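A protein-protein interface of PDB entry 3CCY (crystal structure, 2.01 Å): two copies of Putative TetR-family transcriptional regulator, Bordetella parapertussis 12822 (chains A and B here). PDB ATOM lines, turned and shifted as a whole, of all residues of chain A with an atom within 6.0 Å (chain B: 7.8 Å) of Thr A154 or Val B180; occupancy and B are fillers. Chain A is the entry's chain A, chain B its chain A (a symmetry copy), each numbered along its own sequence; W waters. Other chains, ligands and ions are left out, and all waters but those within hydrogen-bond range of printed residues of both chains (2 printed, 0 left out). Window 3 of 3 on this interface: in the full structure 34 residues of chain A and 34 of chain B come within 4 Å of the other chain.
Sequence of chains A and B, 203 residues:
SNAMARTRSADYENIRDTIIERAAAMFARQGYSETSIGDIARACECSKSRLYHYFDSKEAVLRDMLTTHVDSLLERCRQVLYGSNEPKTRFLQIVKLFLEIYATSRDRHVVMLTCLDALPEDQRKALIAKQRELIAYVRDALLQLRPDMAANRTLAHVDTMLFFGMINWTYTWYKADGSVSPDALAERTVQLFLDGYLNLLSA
OD1 of Asn A152 is in hydrogen-bond range of N of Thr A154 (3.2 Å). The side-chain amide oxygen (OD1) of Asn A152 is in hydrogen-bond range of the backbone NH (N) of Leu A155. OH of Tyr B174 lies within hydrogen-bond range of O of Val B180, at 2.7 Å.
The guanidinium group (NE) of Arg B188 is in salt-bridge range of the side-chain carboxylate (OD1) of Asp A159 (2.8 Å).
Of the 8 printed residues of chain A, 4 touch a printed residue of chain B. Printed residues of chain A that touch a printed residue of chain B: Thr A154, Leu A155, Val A158 and Asp A159. Among the printed residues, 5 pairs touch across the chains. Among the printed residues, Asp or Glu carboxylates within 4 Å of a Lys or Arg side-chain nitrogen of the other chain: Asp A159 with Arg B188 (2.8 Å).
Thr A154 touches Val B180 (CG2 to CG2, 3.8 Å). Leu A155 touches Arg B188. CG2 of Val A158 touches CG2 of Val B180, 3.9 Å away. Val A158 touches Leu B185 (CG1 to CD1, 3.6 Å).
No position is printed for both chains. Of the 5 pairs that touch across the chains among the printed residues, none has its exchanged pair printed and touching as well.
Water W1 bridges the backbone carbonyl oxygen (O) of Trp B173 (2.8 Å) and a ring nitrogen (NE2) of His A157 (3.4 Å). Water W2 lies within hydrogen-bond range of the side-chain hydroxyl (OG1) of Thr A154 (3.0 Å) and the side-chain hydroxyl (OG) of Ser B179 (3.3 Å).
Thr A154 touches just one residue of chain B: Val B180. Of the printed residues of chain A, Val B180 touches Thr A154 and Val A158. Printed residues of chain B within 4 Å of Leu A155: Arg B188 (3.6 Å). Printed residues of chain B within 4 Å of Asp A159: Arg B188 (2.8 Å). Of the printed residues of chain A, Arg B188 touches Leu A155 (3.6 Å) and Asp A159 (2.8 Å). Of the printed residues of chain B, Val A158 touches Val B180 (3.9 Å) and Leu B185 (3.6 Å). Of the printed residues of chain A, Leu B185 touches Val A158. Ala B186 touches none of the printed residues of chain A. Ala B184 touches none of the printed residues of chain A. The nearest residue of chain B that does not touch Thr A154 is Ser B179 (4.2 Å). The nearest residue of chain A that does not touch Val B180 is Leu A155 (4.3 Å).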
ATOM      1  N   ASN A 152      30.267  -5.038  34.979  1.00  0.00           N
ATOM      2  CA  ASN A 152      29.648  -4.033  34.118  1.00  0.00           C
ATOM      3  C   ASN A 152      28.976  -4.677  32.912  1.00  0.00           C
ATOM      4  O   ASN A 152      29.614  -4.889  31.865  1.00  0.00           O
ATOM      5  CB  ASN A 152      30.664  -2.983  33.670  1.00  0.00           C
ATOM      6  CG  ASN A 152      30.007  -1.774  32.990  1.00  0.00           C
ATOM      7  OD1 ASN A 152      28.909  -1.858  32.419  1.00  0.00           O
ATOM      8  ND2 ASN A 152      30.673  -0.633  33.083  1.00  0.00           N
ATOM      9  N   ARG A 153      27.686  -4.975  33.057  1.00  0.00           N
ATOM     10  CA  ARG A 153      26.967  -5.673  32.004  1.00  0.00           C
ATOM     11  C   ARG A 153      26.740  -4.834  30.754  1.00  0.00           C
ATOM     12  O   ARG A 153      26.719  -5.355  29.663  1.00  0.00           O
ATOM     13  CB  ARG A 153      25.662  -6.245  32.544  1.00  0.00           C
ATOM     14  CG  ARG A 153      25.922  -7.520  33.367  1.00  0.00           C
ATOM     15  CD  ARG A 153      24.694  -8.041  34.124  1.00  0.00           C
ATOM     16  NE  ARG A 153      25.096  -9.283  34.771  1.00  0.00           N
ATOM     17  CZ  ARG A 153      25.036 -10.492  34.212  1.00  0.00           C
ATOM     18  NH1 ARG A 153      24.512 -10.680  33.001  1.00  0.00           N
ATOM     19  NH2 ARG A 153      25.476 -11.519  34.898  1.00  0.00           N
ATOM     20  N   THR A 154      26.606  -3.523  30.922  1.00  0.00           N
ATOM     21  CA  THR A 154      26.429  -2.619  29.791  1.00  0.00           C
ATOM     22  C   THR A 154      27.589  -2.703  28.829  1.00  0.00           C
ATOM     23  O   THR A 154      27.394  -2.933  27.646  1.00  0.00           O
ATOM     24  CB  THR A 154      26.232  -1.174  30.268  1.00  0.00           C
ATOM     25  OG1 THR A 154      25.099  -1.131  31.136  1.00  0.00           O
ATOM     26  CG2 THR A 154      25.955  -0.248  29.085  1.00  0.00           C
ATOM     27  N   LEU A 155      28.799  -2.523  29.353  1.00  0.00           N
ATOM     28  CA  LEU A 155      29.996  -2.550  28.556  1.00  0.00           C
ATOM     29  C   LEU A 155      30.353  -3.955  28.106  1.00  0.00           C
ATOM     30  O   LEU A 155      30.920  -4.110  27.043  1.00  0.00           O
ATOM     31  CB  LEU A 155      31.160  -1.872  29.302  1.00  0.00           C
ATOM     32  CG  LEU A 155      31.032  -0.363  29.631  1.00  0.00           C
ATOM     33  CD1 LEU A 155      32.365   0.236  30.118  1.00  0.00           C
ATOM     34  CD2 LEU A 155      30.586   0.394  28.373  1.00  0.00           C
ATOM     35  N   ALA A 156      30.013  -4.984  28.897  1.00  0.00           N
ATOM     36  CA  ALA A 156      30.155  -6.378  28.413  1.00  0.00           C
ATOM     37  C   ALA A 156      29.367  -6.652  27.108  1.00  0.00           C
ATOM     38  O   ALA A 156      29.892  -7.287  26.176  1.00  0.00           O
ATOM     39  CB  ALA A 156      29.783  -7.385  29.501  1.00  0.00           C
ATOM     40  N   HIS A 157      28.121  -6.175  27.047  1.00  0.00           N
ATOM     41  CA  HIS A 157      27.333  -6.223  25.817  1.00  0.00           C
ATOM     42  C   HIS A 157      27.955  -5.394  24.668  1.00  0.00           C
ATOM     43  O   HIS A 157      28.064  -5.897  23.559  1.00  0.00           O
ATOM     44  CB  HIS A 157      25.885  -5.832  26.100  1.00  0.00           C
ATOM     45  CG  HIS A 157      25.026  -5.727  24.880  1.00  0.00           C
ATOM     46  ND1 HIS A 157      24.641  -6.824  24.139  1.00  0.00           N
ATOM     47  CD2 HIS A 157      24.473  -4.646  24.276  1.00  0.00           C
ATOM     48  CE1 HIS A 157      23.879  -6.418  23.136  1.00  0.00           C
ATOM     49  NE2 HIS A 157      23.781  -5.097  23.186  1.00  0.00           N
ATOM     50  N   VAL A 158      28.342  -4.149  24.920  1.00  0.00           N
ATOM     51  CA  VAL A 158      29.127  -3.363  23.940  1.00  0.00           C
ATOM     52  C   VAL A 158      30.348  -4.140  23.433  1.00  0.00           C
ATOM     53  O   VAL A 158      30.525  -4.250  22.230  1.00  0.00           O
ATOM     54  CB  VAL A 158      29.569  -1.959  24.474  1.00  0.00           C
ATOM     55  CG1 VAL A 158      30.401  -1.246  23.435  1.00  0.00           C
ATOM     56  CG2 VAL A 158      28.328  -1.117  24.781  1.00  0.00           C
ATOM     57  N   ASP A 159      31.160  -4.724  24.321  1.00  0.00           N
ATOM     58  CA  ASP A 159      32.398  -5.343  23.839  1.00  0.00           C
ATOM     59  C   ASP A 159      32.083  -6.567  22.966  1.00  0.00           C
ATOM     60  O   ASP A 159      32.749  -6.810  21.947  1.00  0.00           O
ATOM     61  CB  ASP A 159      33.323  -5.755  25.019  1.00  0.00           C
ATOM     62  CG  ASP A 159      33.825  -4.541  25.827  1.00  0.00           C
ATOM     63  OD1 ASP A 159      33.813  -3.415  25.295  1.00  0.00           O
ATOM     64  OD2 ASP A 159      34.241  -4.695  26.993  1.00  0.00           O
ATOM     65  N   TRP B 173      22.526  -3.142  16.254  1.00  0.00           N
ATOM     66  CA  TRP B 173      22.391  -3.362  17.715  1.00  0.00           C
ATOM     67  C   TRP B 173      22.447  -2.081  18.551  1.00  0.00           C
ATOM     68  O   TRP B 173      21.860  -2.007  19.651  1.00  0.00           O
ATOM     69  CB  TRP B 173      23.481  -4.331  18.209  1.00  0.00           C
ATOM     70  CG  TRP B 173      24.945  -3.830  18.098  1.00  0.00           C
ATOM     71  CD1 TRP B 173      25.839  -4.055  17.057  1.00  0.00           C
ATOM     72  CD2 TRP B 173      25.666  -3.084  19.084  1.00  0.00           C
ATOM     73  NE1 TRP B 173      27.061  -3.462  17.343  1.00  0.00           N
ATOM     74  CE2 TRP B 173      26.985  -2.880  18.586  1.00  0.00           C
ATOM     75  CE3 TRP B 173      25.326  -2.560  20.358  1.00  0.00           C
ATOM     76  CZ2 TRP B 173      27.941  -2.169  19.296  1.00  0.00           C
ATOM     77  CZ3 TRP B 173      26.290  -1.851  21.061  1.00  0.00           C
ATOM     78  CH2 TRP B 173      27.587  -1.677  20.524  1.00  0.00           C
ATOM     79  N   TYR B 174      23.178  -1.092  18.052  1.00  0.00           N
ATOM     80  CA  TYR B 174      23.511   0.098  18.864  1.00  0.00           C
ATOM     81  C   TYR B 174      22.484   1.207  18.761  1.00  0.00           C
ATOM     82  O   TYR B 174      22.065   1.580  17.663  1.00  0.00           O
ATOM     83  CB  TYR B 174      24.894   0.631  18.493  1.00  0.00           C
ATOM     84  CG  TYR B 174      25.232   1.932  19.164  1.00  0.00           C
ATOM     85  CD1 TYR B 174      25.460   1.983  20.533  1.00  0.00           C
ATOM     86  CD2 TYR B 174      25.302   3.130  18.415  1.00  0.00           C
ATOM     87  CE1 TYR B 174      25.769   3.191  21.185  1.00  0.00           C
ATOM     88  CE2 TYR B 174      25.575   4.348  19.040  1.00  0.00           C
ATOM     89  CZ  TYR B 174      25.819   4.363  20.427  1.00  0.00           C
ATOM     90  OH  TYR B 174      26.094   5.549  21.047  1.00  0.00           O
ATOM     91  N   LYS B 175      22.061   1.728  19.913  1.00  0.00           N
ATOM     92  CA  LYS B 175      21.134   2.868  19.950  1.00  0.00           C
ATOM     93  C   LYS B 175      21.866   4.112  20.480  1.00  0.00           C
ATOM     94  O   LYS B 175      22.331   4.132  21.624  1.00  0.00           O
ATOM     95  CB  LYS B 175      19.896   2.527  20.775  1.00  0.00           C
ATOM     96  CG  LYS B 175      18.861   1.542  20.121  1.00  0.00           C
ATOM     97  CD  LYS B 175      19.435   0.419  19.214  1.00  0.00           C
ATOM     98  CE  LYS B 175      18.454  -0.798  19.068  1.00  0.00           C
ATOM     99  NZ  LYS B 175      18.808  -1.795  17.970  1.00  0.00           N
ATOM    100  N   ALA B 176      21.998   5.126  19.623  1.00  0.00           N
ATOM    101  CA  ALA B 176      22.780   6.300  19.924  1.00  0.00           C
ATOM    102  C   ALA B 176      22.237   7.193  21.074  1.00  0.00           C
ATOM    103  O   ALA B 176      22.972   8.090  21.567  1.00  0.00           O
ATOM    104  CB  ALA B 176      22.988   7.140  18.657  1.00  0.00           C
ATOM    105  N   ASP B 177      20.977   6.983  21.463  1.00  0.00           N
ATOM    106  CA  ASP B 177      20.371   7.750  22.571  1.00  0.00           C
ATOM    107  C   ASP B 177      20.365   6.967  23.886  1.00  0.00           C
ATOM    108  O   ASP B 177      19.674   7.338  24.847  1.00  0.00           O
ATOM    109  CB  ASP B 177      18.947   8.223  22.202  1.00  0.00           C
ATOM    110  CG  ASP B 177      17.964   7.083  22.022  1.00  0.00           C
ATOM    111  OD1 ASP B 177      18.340   5.884  22.101  1.00  0.00           O
ATOM    112  OD2 ASP B 177      16.772   7.384  21.809  1.00  0.00           O
ATOM    113  N   GLY B 178      21.152   5.896  23.927  1.00  0.00           N
ATOM    114  CA  GLY B 178      21.168   5.004  25.107  1.00  0.00           C
ATOM    115  C   GLY B 178      22.249   5.368  26.105  1.00  0.00           C
ATOM    116  O   GLY B 178      22.866   6.437  26.031  1.00  0.00           O
ATOM    117  N   SER B 179      22.493   4.453  27.025  1.00  0.00           N
ATOM    118  CA  SER B 179      23.479   4.618  28.101  1.00  0.00           C
ATOM    119  C   SER B 179      24.857   5.064  27.608  1.00  0.00           C
ATOM    120  O   SER B 179      25.434   6.078  28.119  1.00  0.00           O
ATOM    121  CB  SER B 179      23.619   3.280  28.813  1.00  0.00           C
ATOM    122  OG  SER B 179      22.476   3.106  29.594  1.00  0.00           O
ATOM    123  N   VAL B 180      25.333   4.364  26.567  1.00  0.00           N
ATOM    124  CA  VAL B 180      26.617   4.600  25.924  1.00  0.00           C
ATOM    125  C   VAL B 180      26.507   5.598  24.738  1.00  0.00           C
ATOM    126  O   VAL B 180      25.853   5.309  23.735  1.00  0.00           O
ATOM    127  CB  VAL B 180      27.230   3.260  25.407  1.00  0.00           C
ATOM    128  CG1 VAL B 180      28.696   3.493  24.893  1.00  0.00           C
ATOM    129  CG2 VAL B 180      27.193   2.210  26.526  1.00  0.00           C
ATOM    130  N   SER B 181      27.166   6.754  24.868  1.00  0.00           N
ATOM    131  CA  SER B 181      27.080   7.820  23.874  1.00  0.00           C
ATOM    132  C   SER B 181      27.905   7.469  22.647  1.00  0.00           C
ATOM    133  O   SER B 181      28.804   6.631  22.735  1.00  0.00           O
ATOM    134  CB  SER B 181      27.587   9.140  24.461  1.00  0.00           C
ATOM    135  OG  SER B 181      29.003   9.086  24.588  1.00  0.00           O
ATOM    136  N   PRO B 182      27.595   8.082  21.484  1.00  0.00           N
ATOM    137  CA  PRO B 182      28.500   7.891  20.334  1.00  0.00           C
ATOM    138  C   PRO B 182      29.991   8.108  20.625  1.00  0.00           C
ATOM    139  O   PRO B 182      30.802   7.257  20.216  1.00  0.00           O
ATOM    140  CB  PRO B 182      27.947   8.863  19.268  1.00  0.00           C
ATOM    141  CG  PRO B 182      26.469   8.845  19.548  1.00  0.00           C
ATOM    142  CD  PRO B 182      26.420   8.898  21.111  1.00  0.00           C
ATOM    143  N   ASP B 183      30.347   9.152  21.385  1.00  0.00           N
ATOM    144  CA  ASP B 183      31.763   9.383  21.740  1.00  0.00           C
ATOM    145  C   ASP B 183      32.324   8.278  22.648  1.00  0.00           C
ATOM    146  O   ASP B 183      33.427   7.828  22.430  1.00  0.00           O
ATOM    147  CB  ASP B 183      32.004  10.744  22.411  1.00  0.00           C
ATOM    148  CG  ASP B 183      32.591  11.771  21.466  1.00  0.00           C
ATOM    149  OD1 ASP B 183      32.385  11.689  20.198  1.00  0.00           O
ATOM    150  OD2 ASP B 183      33.248  12.680  22.021  1.00  0.00           O
ATOM    151  N   ALA B 184      31.580   7.881  23.672  1.00  0.00           N
ATOM    152  CA  ALA B 184      31.951   6.740  24.534  1.00  0.00           C
ATOM    153  C   ALA B 184      32.142   5.454  23.705  1.00  0.00           C
ATOM    154  O   ALA B 184      33.114   4.711  23.894  1.00  0.00           O
ATOM    155  CB  ALA B 184      30.893   6.543  25.670  1.00  0.00           C
ATOM    156  N   LEU B 185      31.242   5.196  22.759  1.00  0.00           N
ATOM    157  CA  LEU B 185      31.365   3.969  21.960  1.00  0.00           C
ATOM    158  C   LEU B 185      32.660   4.025  21.111  1.00  0.00           C
ATOM    159  O   LEU B 185      33.383   3.013  20.967  1.00  0.00           O
ATOM    160  CB  LEU B 185      30.106   3.746  21.092  1.00  0.00           C
ATOM    161  CG  LEU B 185      30.187   2.565  20.127  1.00  0.00           C
ATOM    162  CD1 LEU B 185      30.331   1.263  20.919  1.00  0.00           C
ATOM    163  CD2 LEU B 185      28.911   2.489  19.224  1.00  0.00           C
ATOM    164  N   ALA B 186      32.949   5.205  20.559  1.00  0.00           N
ATOM    165  CA  ALA B 186      34.114   5.418  19.707  1.00  0.00           C
ATOM    166  C   ALA B 186      35.392   5.198  20.506  1.00  0.00           C
ATOM    167  O   ALA B 186      36.278   4.473  20.034  1.00  0.00           O
ATOM    168  CB  ALA B 186      34.121   6.881  19.091  1.00  0.00           C
ATOM    169  N   ARG B 188      35.801   3.507  23.314  1.00  0.00           N
ATOM    170  CA  ARG B 188      35.825   2.075  23.601  1.00  0.00           C
ATOM    171  C   ARG B 188      36.316   1.247  22.403  1.00  0.00           C
ATOM    172  O   ARG B 188      37.170   0.383  22.566  1.00  0.00           O
ATOM    173  CB  ARG B 188      34.420   1.580  23.927  1.00  0.00           C
ATOM    174  CG  ARG B 188      34.391   0.096  24.469  1.00  0.00           C
ATOM    175  CD  ARG B 188      34.973   0.082  25.841  1.00  0.00           C
ATOM    176  NE  ARG B 188      34.747  -1.166  26.574  1.00  0.00           N
ATOM    177  CZ  ARG B 188      35.030  -1.303  27.865  1.00  0.00           C
ATOM    178  NH1 ARG B 188      35.519  -0.265  28.532  1.00  0.00           N
ATOM    179  NH2 ARG B 188      34.842  -2.449  28.479  1.00  0.00           N
HETATM  180  O   HOH W   1      22.221  -2.141  22.458  1.00  0.00           O
HETATM  181  O   HOH W   2      22.454  -0.177  30.004  1.00  0.00           O
